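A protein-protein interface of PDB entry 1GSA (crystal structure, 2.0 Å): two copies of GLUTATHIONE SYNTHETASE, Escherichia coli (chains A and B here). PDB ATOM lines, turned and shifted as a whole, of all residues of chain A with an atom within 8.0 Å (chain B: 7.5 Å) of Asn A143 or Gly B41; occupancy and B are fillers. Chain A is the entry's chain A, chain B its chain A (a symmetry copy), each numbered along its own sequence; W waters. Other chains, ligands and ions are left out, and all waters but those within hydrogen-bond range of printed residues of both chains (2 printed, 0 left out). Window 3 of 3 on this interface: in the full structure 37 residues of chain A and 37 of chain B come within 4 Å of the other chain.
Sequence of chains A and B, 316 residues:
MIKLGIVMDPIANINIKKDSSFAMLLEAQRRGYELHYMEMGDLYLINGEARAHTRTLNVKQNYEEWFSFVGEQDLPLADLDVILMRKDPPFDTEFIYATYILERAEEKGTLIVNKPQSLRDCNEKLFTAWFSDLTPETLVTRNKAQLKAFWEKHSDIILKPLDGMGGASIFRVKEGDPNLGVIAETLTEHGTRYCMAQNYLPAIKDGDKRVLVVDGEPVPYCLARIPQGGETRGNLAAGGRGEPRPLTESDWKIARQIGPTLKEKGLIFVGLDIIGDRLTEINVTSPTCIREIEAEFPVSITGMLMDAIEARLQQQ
Water W1 lies within hydrogen-bond range of the backbone carbonyl oxygen (O) of Leu B43 (2.6 Å), the backbone carbonyl oxygen (O) of Gly B41 (2.6 Å), the backbone NH (N) of Arg A142 (3.0 Å), the side-chain hydroxyl (OG1) of Thr A141 (3.3 Å) and the side-chain amide nitrogen (ND2) of Asn A143 (3.3 Å). Water W2 lies within hydrogen-bond range of OE1 of Gln A146, ND2 of Asn A143 and O of Asp B42.
Printed residues of chain B within 4 Å of Asn A143: Gly B41 (2.8 Å). Of chain A, only Arg A142 and Asn A143 come within 4 Å of Gly B41. Printed residues of chain B within 4 Å of Leu A139: Tyr B44 (3.9 Å). Printed residues of chain B within 4 Å of Tyr A194: Met B40 and Leu B43. Printed residues of chain A within 4 Å of Tyr B44: Leu A139 (3.9 Å), Val A140 (3.2 Å) and Gln A146 (3.6 Å). Leu A180 touches none of the printed residues of chain B. The nearest residue of chain B that does not touch Asn A143 is Asp B42 (4.8 Å).
OG1 of Thr A141 is in hydrogen-bond range of OE1 of Gln A146 (3.1 Å). The side-chain hydroxyl (OG1) of Thr A141 sits at hydrogen-bond distance from the backbone NH (N) of Asn A143, at 3.2 Å. The side-chain amide oxygen of Gln A146 lies within hydrogen-bond range of the side-chain amide nitrogen of Asn A143, 3.0 Å away. O of Thr A192 lies close to NH2 of Arg A142 (3.3 Å).
No position is printed for both chains. Of the 8 pairs that touch across the chains among the printed residues, none has its exchanged pair printed and touching as well.
Tyr B44 touches Leu A139 (CD2 to CD1, 3.9 Å). O of Val A140 touches CB of Tyr B44 (3.2 Å). CB of Met B40 touches NH1 of Arg A142 (3.3 Å). CD of Arg A142 touches CA of Gly B41, 3.7 Å away. Gln A146 touches Tyr B44 (NE2 to CD2, 3.6 Å). Tyr A194 touches Leu B43.
The side-chain amide nitrogen (ND2) of Asn A143 lies within hydrogen-bond range of the backbone carbonyl oxygen (O) of Gly B41 (2.8 Å). The backbone carbonyl oxygen of Met B40 lies within hydrogen-bond range of the side-chain hydroxyl of Tyr A194 (2.8 Å).
Among the printed residues, 8 pairs touch across the chains. Among the printed residues, no Asp or Glu carboxylate lies within 4 Å of a Lys or Arg side-chain nitrogen of the other chain.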
ATOM      1  N   LEU A 139       7.018 -24.215   7.177  1.00  0.00           N
ATOM      2  CA  LEU A 139       6.572 -22.884   7.476  1.00  0.00           C
ATOM      3  C   LEU A 139       6.369 -22.863   8.975  1.00  0.00           C
ATOM      4  O   LEU A 139       5.747 -23.797   9.497  1.00  0.00           O
ATOM      5  CB  LEU A 139       5.234 -22.606   6.758  1.00  0.00           C
ATOM      6  CG  LEU A 139       4.383 -21.350   7.022  1.00  0.00           C
ATOM      7  CD1 LEU A 139       5.047 -20.104   6.482  1.00  0.00           C
ATOM      8  CD2 LEU A 139       3.047 -21.505   6.317  1.00  0.00           C
ATOM      9  N   VAL A 140       6.856 -21.841   9.682  1.00  0.00           N
ATOM     10  CA  VAL A 140       6.604 -21.677  11.092  1.00  0.00           C
ATOM     11  C   VAL A 140       5.839 -20.369  11.162  1.00  0.00           C
ATOM     12  O   VAL A 140       6.391 -19.355  10.756  1.00  0.00           O
ATOM     13  CB  VAL A 140       7.957 -21.624  11.838  1.00  0.00           C
ATOM     14  CG1 VAL A 140       7.811 -21.263  13.311  1.00  0.00           C
ATOM     15  CG2 VAL A 140       8.578 -23.002  11.689  1.00  0.00           C
ATOM     16  N   THR A 141       4.602 -20.312  11.638  1.00  0.00           N
ATOM     17  CA  THR A 141       3.859 -19.068  11.605  1.00  0.00           C
ATOM     18  C   THR A 141       2.807 -19.067  12.694  1.00  0.00           C
ATOM     19  O   THR A 141       2.558 -20.133  13.250  1.00  0.00           O
ATOM     20  CB  THR A 141       3.209 -18.932  10.191  1.00  0.00           C
ATOM     21  OG1 THR A 141       2.550 -17.672  10.126  1.00  0.00           O
ATOM     22  CG2 THR A 141       2.174 -20.017   9.908  1.00  0.00           C
ATOM     23  N   ARG A 142       2.227 -17.899  13.026  1.00  0.00           N
ATOM     24  CA  ARG A 142       1.076 -17.756  13.908  1.00  0.00           C
ATOM     25  C   ARG A 142      -0.204 -17.500  13.118  1.00  0.00           C
ATOM     26  O   ARG A 142      -1.320 -17.573  13.645  1.00  0.00           O
ATOM     27  CB  ARG A 142       1.225 -16.587  14.827  1.00  0.00           C
ATOM     28  CG  ARG A 142       2.228 -16.808  15.942  1.00  0.00           C
ATOM     29  CD  ARG A 142       2.350 -15.629  16.892  1.00  0.00           C
ATOM     30  NE  ARG A 142       3.243 -15.934  18.010  1.00  0.00           N
ATOM     31  CZ  ARG A 142       3.425 -15.117  19.056  1.00  0.00           C
ATOM     32  NH1 ARG A 142       2.793 -13.965  19.172  1.00  0.00           N
ATOM     33  NH2 ARG A 142       4.302 -15.428  19.989  1.00  0.00           N
ATOM     34  N   ASN A 143      -0.100 -17.232  11.819  1.00  0.00           N
ATOM     35  CA  ASN A 143      -1.232 -16.765  11.037  1.00  0.00           C
ATOM     36  C   ASN A 143      -1.843 -17.856  10.196  1.00  0.00           C
ATOM     37  O   ASN A 143      -1.229 -18.458   9.316  1.00  0.00           O
ATOM     38  CB  ASN A 143      -0.829 -15.611  10.099  1.00  0.00           C
ATOM     39  CG  ASN A 143      -0.068 -14.539  10.865  1.00  0.00           C
ATOM     40  OD1 ASN A 143      -0.556 -13.898  11.817  1.00  0.00           O
ATOM     41  ND2 ASN A 143       1.205 -14.382  10.517  1.00  0.00           N
ATOM     42  N   LYS A 144      -3.109 -18.061  10.514  1.00  0.00           N
ATOM     43  CA  LYS A 144      -4.000 -18.965   9.842  1.00  0.00           C
ATOM     44  C   LYS A 144      -4.009 -18.682   8.346  1.00  0.00           C
ATOM     45  O   LYS A 144      -4.064 -19.610   7.542  1.00  0.00           O
ATOM     46  CB  LYS A 144      -5.398 -18.789  10.400  1.00  0.00           C
ATOM     47  CG  LYS A 144      -6.367 -19.786   9.757  1.00  0.00           C
ATOM     48  CD  LYS A 144      -7.818 -19.413   9.979  1.00  0.00           C
ATOM     49  CE  LYS A 144      -8.130 -19.610  11.435  1.00  0.00           C
ATOM     50  NZ  LYS A 144      -9.487 -19.174  11.635  1.00  0.00           N
ATOM     51  N   ALA A 145      -3.903 -17.424   7.936  1.00  0.00           N
ATOM     52  CA  ALA A 145      -3.904 -17.074   6.518  1.00  0.00           C
ATOM     53  C   ALA A 145      -2.755 -17.712   5.777  1.00  0.00           C
ATOM     54  O   ALA A 145      -2.920 -18.232   4.670  1.00  0.00           O
ATOM     55  CB  ALA A 145      -3.780 -15.573   6.320  1.00  0.00           C
ATOM     56  N   GLN A 146      -1.583 -17.744   6.425  1.00  0.00           N
ATOM     57  CA  GLN A 146      -0.396 -18.344   5.825  1.00  0.00           C
ATOM     58  C   GLN A 146      -0.512 -19.856   5.840  1.00  0.00           C
ATOM     59  O   GLN A 146      -0.035 -20.517   4.927  1.00  0.00           O
ATOM     60  CB  GLN A 146       0.867 -17.956   6.576  1.00  0.00           C
ATOM     61  CG  GLN A 146       1.012 -16.452   6.732  1.00  0.00           C
ATOM     62  CD  GLN A 146       2.414 -16.032   7.108  1.00  0.00           C
ATOM     63  OE1 GLN A 146       2.663 -15.323   8.085  1.00  0.00           O
ATOM     64  NE2 GLN A 146       3.406 -16.400   6.323  1.00  0.00           N
ATOM     65  N   LEU A 147      -1.159 -20.423   6.848  1.00  0.00           N
ATOM     66  CA  LEU A 147      -1.345 -21.843   6.932  1.00  0.00           C
ATOM     67  C   LEU A 147      -2.285 -22.284   5.833  1.00  0.00           C
ATOM     68  O   LEU A 147      -2.001 -23.291   5.205  1.00  0.00           O
ATOM     69  CB  LEU A 147      -1.915 -22.214   8.318  1.00  0.00           C
ATOM     70  CG  LEU A 147      -0.990 -22.080   9.536  1.00  0.00           C
ATOM     71  CD1 LEU A 147      -1.723 -22.453  10.779  1.00  0.00           C
ATOM     72  CD2 LEU A 147       0.174 -23.031   9.405  1.00  0.00           C
ATOM     73  N   LYS A 148      -3.344 -21.541   5.539  1.00  0.00           N
ATOM     74  CA  LYS A 148      -4.335 -21.850   4.513  1.00  0.00           C
ATOM     75  C   LYS A 148      -3.703 -21.797   3.150  1.00  0.00           C
ATOM     76  O   LYS A 148      -3.875 -22.698   2.326  1.00  0.00           O
ATOM     77  CB  LYS A 148      -5.474 -20.857   4.539  1.00  0.00           C
ATOM     78  CG  LYS A 148      -6.594 -21.358   3.666  1.00  0.00           C
ATOM     79  CD  LYS A 148      -7.936 -20.781   4.083  1.00  0.00           C
ATOM     80  CE  LYS A 148      -8.434 -19.660   3.154  1.00  0.00           C
ATOM     81  NZ  LYS A 148      -8.547 -20.105   1.767  1.00  0.00           N
ATOM     82  N   ALA A 149      -2.941 -20.743   2.907  1.00  0.00           N
ATOM     83  CA  ALA A 149      -2.215 -20.626   1.664  1.00  0.00           C
ATOM     84  C   ALA A 149      -1.214 -21.773   1.508  1.00  0.00           C
ATOM     85  O   ALA A 149      -1.199 -22.361   0.428  1.00  0.00           O
ATOM     86  CB  ALA A 149      -1.506 -19.280   1.627  1.00  0.00           C
ATOM     87  N   PHE A 150      -0.417 -22.205   2.492  1.00  0.00           N
ATOM     88  CA  PHE A 150       0.502 -23.340   2.376  1.00  0.00           C
ATOM     89  C   PHE A 150      -0.211 -24.647   2.075  1.00  0.00           C
ATOM     90  O   PHE A 150       0.311 -25.533   1.378  1.00  0.00           O
ATOM     91  CB  PHE A 150       1.280 -23.462   3.676  1.00  0.00           C
ATOM     92  CG  PHE A 150       2.477 -24.394   3.733  1.00  0.00           C
ATOM     93  CD1 PHE A 150       3.717 -23.995   3.240  1.00  0.00           C
ATOM     94  CD2 PHE A 150       2.336 -25.655   4.311  1.00  0.00           C
ATOM     95  CE1 PHE A 150       4.810 -24.853   3.323  1.00  0.00           C
ATOM     96  CE2 PHE A 150       3.434 -26.514   4.394  1.00  0.00           C
ATOM     97  CZ  PHE A 150       4.663 -26.110   3.900  1.00  0.00           C
ATOM     98  N   LEU A 180      -9.391 -27.066   8.691  1.00  0.00           N
ATOM     99  CA  LEU A 180      -8.167 -26.265   8.683  1.00  0.00           C
ATOM    100  C   LEU A 180      -8.298 -25.164   9.711  1.00  0.00           C
ATOM    101  O   LEU A 180      -7.458 -25.071  10.594  1.00  0.00           O
ATOM    102  CB  LEU A 180      -7.945 -25.666   7.304  1.00  0.00           C
ATOM    103  CG  LEU A 180      -6.606 -25.041   6.859  1.00  0.00           C
ATOM    104  CD1 LEU A 180      -6.586 -23.568   7.234  1.00  0.00           C
ATOM    105  CD2 LEU A 180      -5.454 -25.791   7.470  1.00  0.00           C
ATOM    106  N   ALA A 184      -5.920 -24.694  13.019  1.00  0.00           N
ATOM    107  CA  ALA A 184      -5.007 -23.589  13.119  1.00  0.00           C
ATOM    108  C   ALA A 184      -5.373 -22.832  14.372  1.00  0.00           C
ATOM    109  O   ALA A 184      -4.456 -22.543  15.123  1.00  0.00           O
ATOM    110  CB  ALA A 184      -5.148 -22.668  11.920  1.00  0.00           C
ATOM    111  N   THR A 188      -2.253 -22.560  17.093  1.00  0.00           N
ATOM    112  CA  THR A 188      -1.663 -21.261  17.322  1.00  0.00           C
ATOM    113  C   THR A 188      -2.346 -20.570  18.484  1.00  0.00           C
ATOM    114  O   THR A 188      -2.039 -19.417  18.751  1.00  0.00           O
ATOM    115  CB  THR A 188      -1.814 -20.439  16.051  1.00  0.00           C
ATOM    116  OG1 THR A 188      -3.222 -20.321  15.847  1.00  0.00           O
ATOM    117  CG2 THR A 188      -1.131 -21.056  14.819  1.00  0.00           C
ATOM    118  N   HIS A 190      -5.378 -19.260  18.752  1.00  0.00           N
ATOM    119  CA  HIS A 190      -5.950 -18.081  18.121  1.00  0.00           C
ATOM    120  C   HIS A 190      -4.906 -17.044  17.743  1.00  0.00           C
ATOM    121  O   HIS A 190      -5.046 -15.842  17.914  1.00  0.00           O
ATOM    122  CB  HIS A 190      -7.030 -17.466  19.036  1.00  0.00           C
ATOM    123  CG  HIS A 190      -8.212 -18.421  19.122  1.00  0.00           C
ATOM    124  ND1 HIS A 190      -8.334 -19.513  19.887  1.00  0.00           N
ATOM    125  CD2 HIS A 190      -9.371 -18.301  18.372  1.00  0.00           C
ATOM    126  CE1 HIS A 190      -9.507 -20.054  19.636  1.00  0.00           C
ATOM    127  NE2 HIS A 190     -10.125 -19.322  18.726  1.00  0.00           N
ATOM    128  N   GLY A 191      -3.812 -17.545  17.223  1.00  0.00           N
ATOM    129  CA  GLY A 191      -2.810 -16.687  16.640  1.00  0.00           C
ATOM    130  C   GLY A 191      -1.831 -16.125  17.619  1.00  0.00           C
ATOM    131  O   GLY A 191      -1.176 -15.151  17.269  1.00  0.00           O
ATOM    132  N   THR A 192      -1.696 -16.689  18.808  1.00  0.00           N
ATOM    133  CA  THR A 192      -0.777 -16.175  19.797  1.00  0.00           C
ATOM    134  C   THR A 192       0.413 -17.090  19.991  1.00  0.00           C
ATOM    135  O   THR A 192       1.345 -16.735  20.702  1.00  0.00           O
ATOM    136  CB  THR A 192      -1.527 -15.974  21.118  1.00  0.00           C
ATOM    137  OG1 THR A 192      -2.007 -17.229  21.549  1.00  0.00           O
ATOM    138  CG2 THR A 192      -2.721 -15.083  20.975  1.00  0.00           C
ATOM    139  N   ARG A 193       0.416 -18.279  19.390  1.00  0.00           N
ATOM    140  CA  ARG A 193       1.528 -19.209  19.429  1.00  0.00           C
ATOM    141  C   ARG A 193       1.928 -19.635  18.037  1.00  0.00           C
ATOM    142  O   ARG A 193       1.084 -19.827  17.176  1.00  0.00           O
ATOM    143  CB  ARG A 193       1.210 -20.489  20.137  1.00  0.00           C
ATOM    144  CG  ARG A 193       0.886 -20.152  21.542  1.00  0.00           C
ATOM    145  CD  ARG A 193       0.929 -21.355  22.444  1.00  0.00           C
ATOM    146  NE  ARG A 193       0.591 -20.786  23.742  1.00  0.00           N
ATOM    147  CZ  ARG A 193       1.434 -20.772  24.779  1.00  0.00           C
ATOM    148  NH1 ARG A 193       2.669 -21.306  24.716  1.00  0.00           N
ATOM    149  NH2 ARG A 193       1.037 -20.145  25.890  1.00  0.00           N
ATOM    150  N   TYR A 194       3.210 -19.811  17.787  1.00  0.00           N
ATOM    151  CA  TYR A 194       3.733 -20.318  16.516  1.00  0.00           C
ATOM    152  C   TYR A 194       3.457 -21.806  16.405  1.00  0.00           C
ATOM    153  O   TYR A 194       3.468 -22.487  17.434  1.00  0.00           O
ATOM    154  CB  TYR A 194       5.269 -20.176  16.384  1.00  0.00           C
ATOM    155  CG  TYR A 194       5.835 -18.767  16.375  1.00  0.00           C
ATOM    156  CD1 TYR A 194       5.588 -17.897  15.313  1.00  0.00           C
ATOM    157  CD2 TYR A 194       6.547 -18.318  17.482  1.00  0.00           C
ATOM    158  CE1 TYR A 194       6.037 -16.569  15.368  1.00  0.00           C
ATOM    159  CE2 TYR A 194       6.994 -16.998  17.538  1.00  0.00           C
ATOM    160  CZ  TYR A 194       6.730 -16.125  16.484  1.00  0.00           C
ATOM    161  OH  TYR A 194       7.110 -14.810  16.591  1.00  0.00           O
ATOM    162  N   CYS A 195       3.188 -22.314  15.208  1.00  0.00           N
ATOM    163  CA  CYS A 195       3.144 -23.749  14.964  1.00  0.00           C
ATOM    164  C   CYS A 195       3.928 -23.999  13.682  1.00  0.00           C
ATOM    165  O   CYS A 195       4.403 -23.053  13.026  1.00  0.00           O
ATOM    166  CB  CYS A 195       1.729 -24.269  14.782  1.00  0.00           C
ATOM    167  SG  CYS A 195       0.874 -23.677  13.319  1.00  0.00           S
ATOM    168  N   VAL B   7      10.594  -5.171  16.758  1.00  0.00           N
ATOM    169  CA  VAL B   7       9.560  -6.124  17.112  1.00  0.00           C
ATOM    170  C   VAL B   7       9.113  -5.621  18.485  1.00  0.00           C
ATOM    171  O   VAL B   7       9.935  -5.448  19.388  1.00  0.00           O
ATOM    172  CB  VAL B   7      10.142  -7.564  17.158  1.00  0.00           C
ATOM    173  CG1 VAL B   7       9.050  -8.561  17.540  1.00  0.00           C
ATOM    174  CG2 VAL B   7      10.631  -7.985  15.771  1.00  0.00           C
ATOM    175  N   MET B   8       7.838  -5.313  18.707  1.00  0.00           N
ATOM    176  CA  MET B   8       7.420  -4.801  19.982  1.00  0.00           C
ATOM    177  C   MET B   8       5.981  -5.163  20.241  1.00  0.00           C
ATOM    178  O   MET B   8       5.292  -5.723  19.385  1.00  0.00           O
ATOM    179  CB  MET B   8       7.614  -3.287  19.992  1.00  0.00           C
ATOM    180  CG  MET B   8       6.919  -2.521  18.877  1.00  0.00           C
ATOM    181  SD  MET B   8       7.098  -0.746  19.091  1.00  0.00           S
ATOM    182  CE  MET B   8       6.113  -0.594  20.556  1.00  0.00           C
ATOM    183  N   MET B  38       7.053  -4.298  13.524  1.00  0.00           N
ATOM    184  CA  MET B  38       6.585  -5.667  13.522  1.00  0.00           C
ATOM    185  C   MET B  38       6.068  -6.041  14.882  1.00  0.00           C
ATOM    186  O   MET B  38       6.489  -5.487  15.873  1.00  0.00           O
ATOM    187  CB  MET B  38       7.695  -6.648  13.183  1.00  0.00           C
ATOM    188  CG  MET B  38       8.179  -6.546  11.769  1.00  0.00           C
ATOM    189  SD  MET B  38       9.808  -7.271  11.579  1.00  0.00           S
ATOM    190  CE  MET B  38      10.836  -5.874  11.843  1.00  0.00           C
ATOM    191  N   GLU B  39       5.141  -6.959  14.994  1.00  0.00           N
ATOM    192  CA  GLU B  39       4.691  -7.549  16.247  1.00  0.00           C
ATOM    193  C   GLU B  39       5.057  -9.021  16.103  1.00  0.00           C
ATOM    194  O   GLU B  39       5.303  -9.468  14.976  1.00  0.00           O
ATOM    195  CB  GLU B  39       3.201  -7.416  16.404  1.00  0.00           C
ATOM    196  CG  GLU B  39       2.812  -5.956  16.568  1.00  0.00           C
ATOM    197  CD  GLU B  39       1.334  -5.636  16.688  1.00  0.00           C
ATOM    198  OE1 GLU B  39       0.515  -6.524  16.894  1.00  0.00           O
ATOM    199  OE2 GLU B  39       0.975  -4.471  16.562  1.00  0.00           O
ATOM    200  N   MET B  40       5.070  -9.836  17.156  1.00  0.00           N
ATOM    201  CA  MET B  40       5.497 -11.235  17.137  1.00  0.00           C
ATOM    202  C   MET B  40       4.817 -12.078  16.082  1.00  0.00           C
ATOM    203  O   MET B  40       5.431 -12.923  15.492  1.00  0.00           O
ATOM    204  CB  MET B  40       5.235 -11.908  18.486  1.00  0.00           C
ATOM    205  CG  MET B  40       5.999 -11.316  19.639  1.00  0.00           C
ATOM    206  SD  MET B  40       7.625 -12.047  19.771  1.00  0.00           S
ATOM    207  CE  MET B  40       7.056 -13.457  20.677  1.00  0.00           C
ATOM    208  N   GLY B  41       3.552 -11.847  15.782  1.00  0.00           N
ATOM    209  CA  GLY B  41       2.780 -12.624  14.813  1.00  0.00           C
ATOM    210  C   GLY B  41       3.152 -12.354  13.364  1.00  0.00           C
ATOM    211  O   GLY B  41       2.783 -13.128  12.490  1.00  0.00           O
ATOM    212  N   ASP B  42       3.887 -11.287  13.058  1.00  0.00           N
ATOM    213  CA  ASP B  42       4.293 -10.918  11.718  1.00  0.00           C
ATOM    214  C   ASP B  42       5.510 -11.655  11.206  1.00  0.00           C
ATOM    215  O   ASP B  42       5.828 -11.644  10.009  1.00  0.00           O
ATOM    216  CB  ASP B  42       4.590  -9.439  11.686  1.00  0.00           C
ATOM    217  CG  ASP B  42       3.431  -8.471  11.845  1.00  0.00           C
ATOM    218  OD1 ASP B  42       2.340  -8.714  11.358  1.00  0.00           O
ATOM    219  OD2 ASP B  42       3.624  -7.423  12.438  1.00  0.00           O
ATOM    220  N   LEU B  43       6.276 -12.240  12.113  1.00  0.00           N
ATOM    221  CA  LEU B  43       7.515 -12.910  11.772  1.00  0.00           C
ATOM    222  C   LEU B  43       7.212 -14.371  11.483  1.00  0.00           C
ATOM    223  O   LEU B  43       6.334 -14.995  12.115  1.00  0.00           O
ATOM    224  CB  LEU B  43       8.536 -12.900  12.917  1.00  0.00           C
ATOM    225  CG  LEU B  43       8.771 -11.653  13.734  1.00  0.00           C
ATOM    226  CD1 LEU B  43       9.617 -12.015  14.953  1.00  0.00           C
ATOM    227  CD2 LEU B  43       9.404 -10.602  12.874  1.00  0.00           C
ATOM    228  N   TYR B  44       7.944 -14.929  10.533  1.00  0.00           N
ATOM    229  CA  TYR B  44       7.769 -16.315  10.219  1.00  0.00           C
ATOM    230  C   TYR B  44       9.025 -16.841   9.570  1.00  0.00           C
ATOM    231  O   TYR B  44       9.962 -16.092   9.279  1.00  0.00           O
ATOM    232  CB  TYR B  44       6.557 -16.475   9.299  1.00  0.00           C
ATOM    233  CG  TYR B  44       6.603 -15.871   7.916  1.00  0.00           C
ATOM    234  CD1 TYR B  44       6.285 -14.528   7.690  1.00  0.00           C
ATOM    235  CD2 TYR B  44       6.945 -16.717   6.858  1.00  0.00           C
ATOM    236  CE1 TYR B  44       6.297 -14.042   6.377  1.00  0.00           C
ATOM    237  CE2 TYR B  44       6.950 -16.233   5.554  1.00  0.00           C
ATOM    238  CZ  TYR B  44       6.624 -14.908   5.323  1.00  0.00           C
ATOM    239  OH  TYR B  44       6.619 -14.480   4.013  1.00  0.00           O
ATOM    240  N   ALA B  52       9.060 -11.327   7.285  1.00  0.00           N
ATOM    241  CA  ALA B  52       8.033 -10.694   8.085  1.00  0.00           C
ATOM    242  C   ALA B  52       7.159  -9.777   7.268  1.00  0.00           C
ATOM    243  O   ALA B  52       7.545  -9.219   6.241  1.00  0.00           O
ATOM    244  CB  ALA B  52       8.615  -9.827   9.193  1.00  0.00           C
ATOM    245  N   HIS B  53       5.946  -9.610   7.713  1.00  0.00           N
ATOM    246  CA  HIS B  53       5.072  -8.622   7.143  1.00  0.00           C
ATOM    247  C   HIS B  53       5.411  -7.380   7.950  1.00  0.00           C
ATOM    248  O   HIS B  53       5.180  -7.366   9.160  1.00  0.00           O
ATOM    249  CB  HIS B  53       3.631  -9.022   7.363  1.00  0.00           C
ATOM    250  CG  HIS B  53       2.651  -7.848   7.405  1.00  0.00           C
ATOM    251  ND1 HIS B  53       1.948  -7.446   8.466  1.00  0.00           N
ATOM    252  CD2 HIS B  53       2.338  -7.009   6.349  1.00  0.00           C
ATOM    253  CE1 HIS B  53       1.231  -6.409   8.110  1.00  0.00           C
ATOM    254  NE2 HIS B  53       1.472  -6.149   6.840  1.00  0.00           N
HETATM  255  O   HOH W   1       3.829 -15.482  12.245  1.00  0.00           O
HETATM  256  O   HOH W   2       3.040 -12.695   8.791  1.00  0.00           O
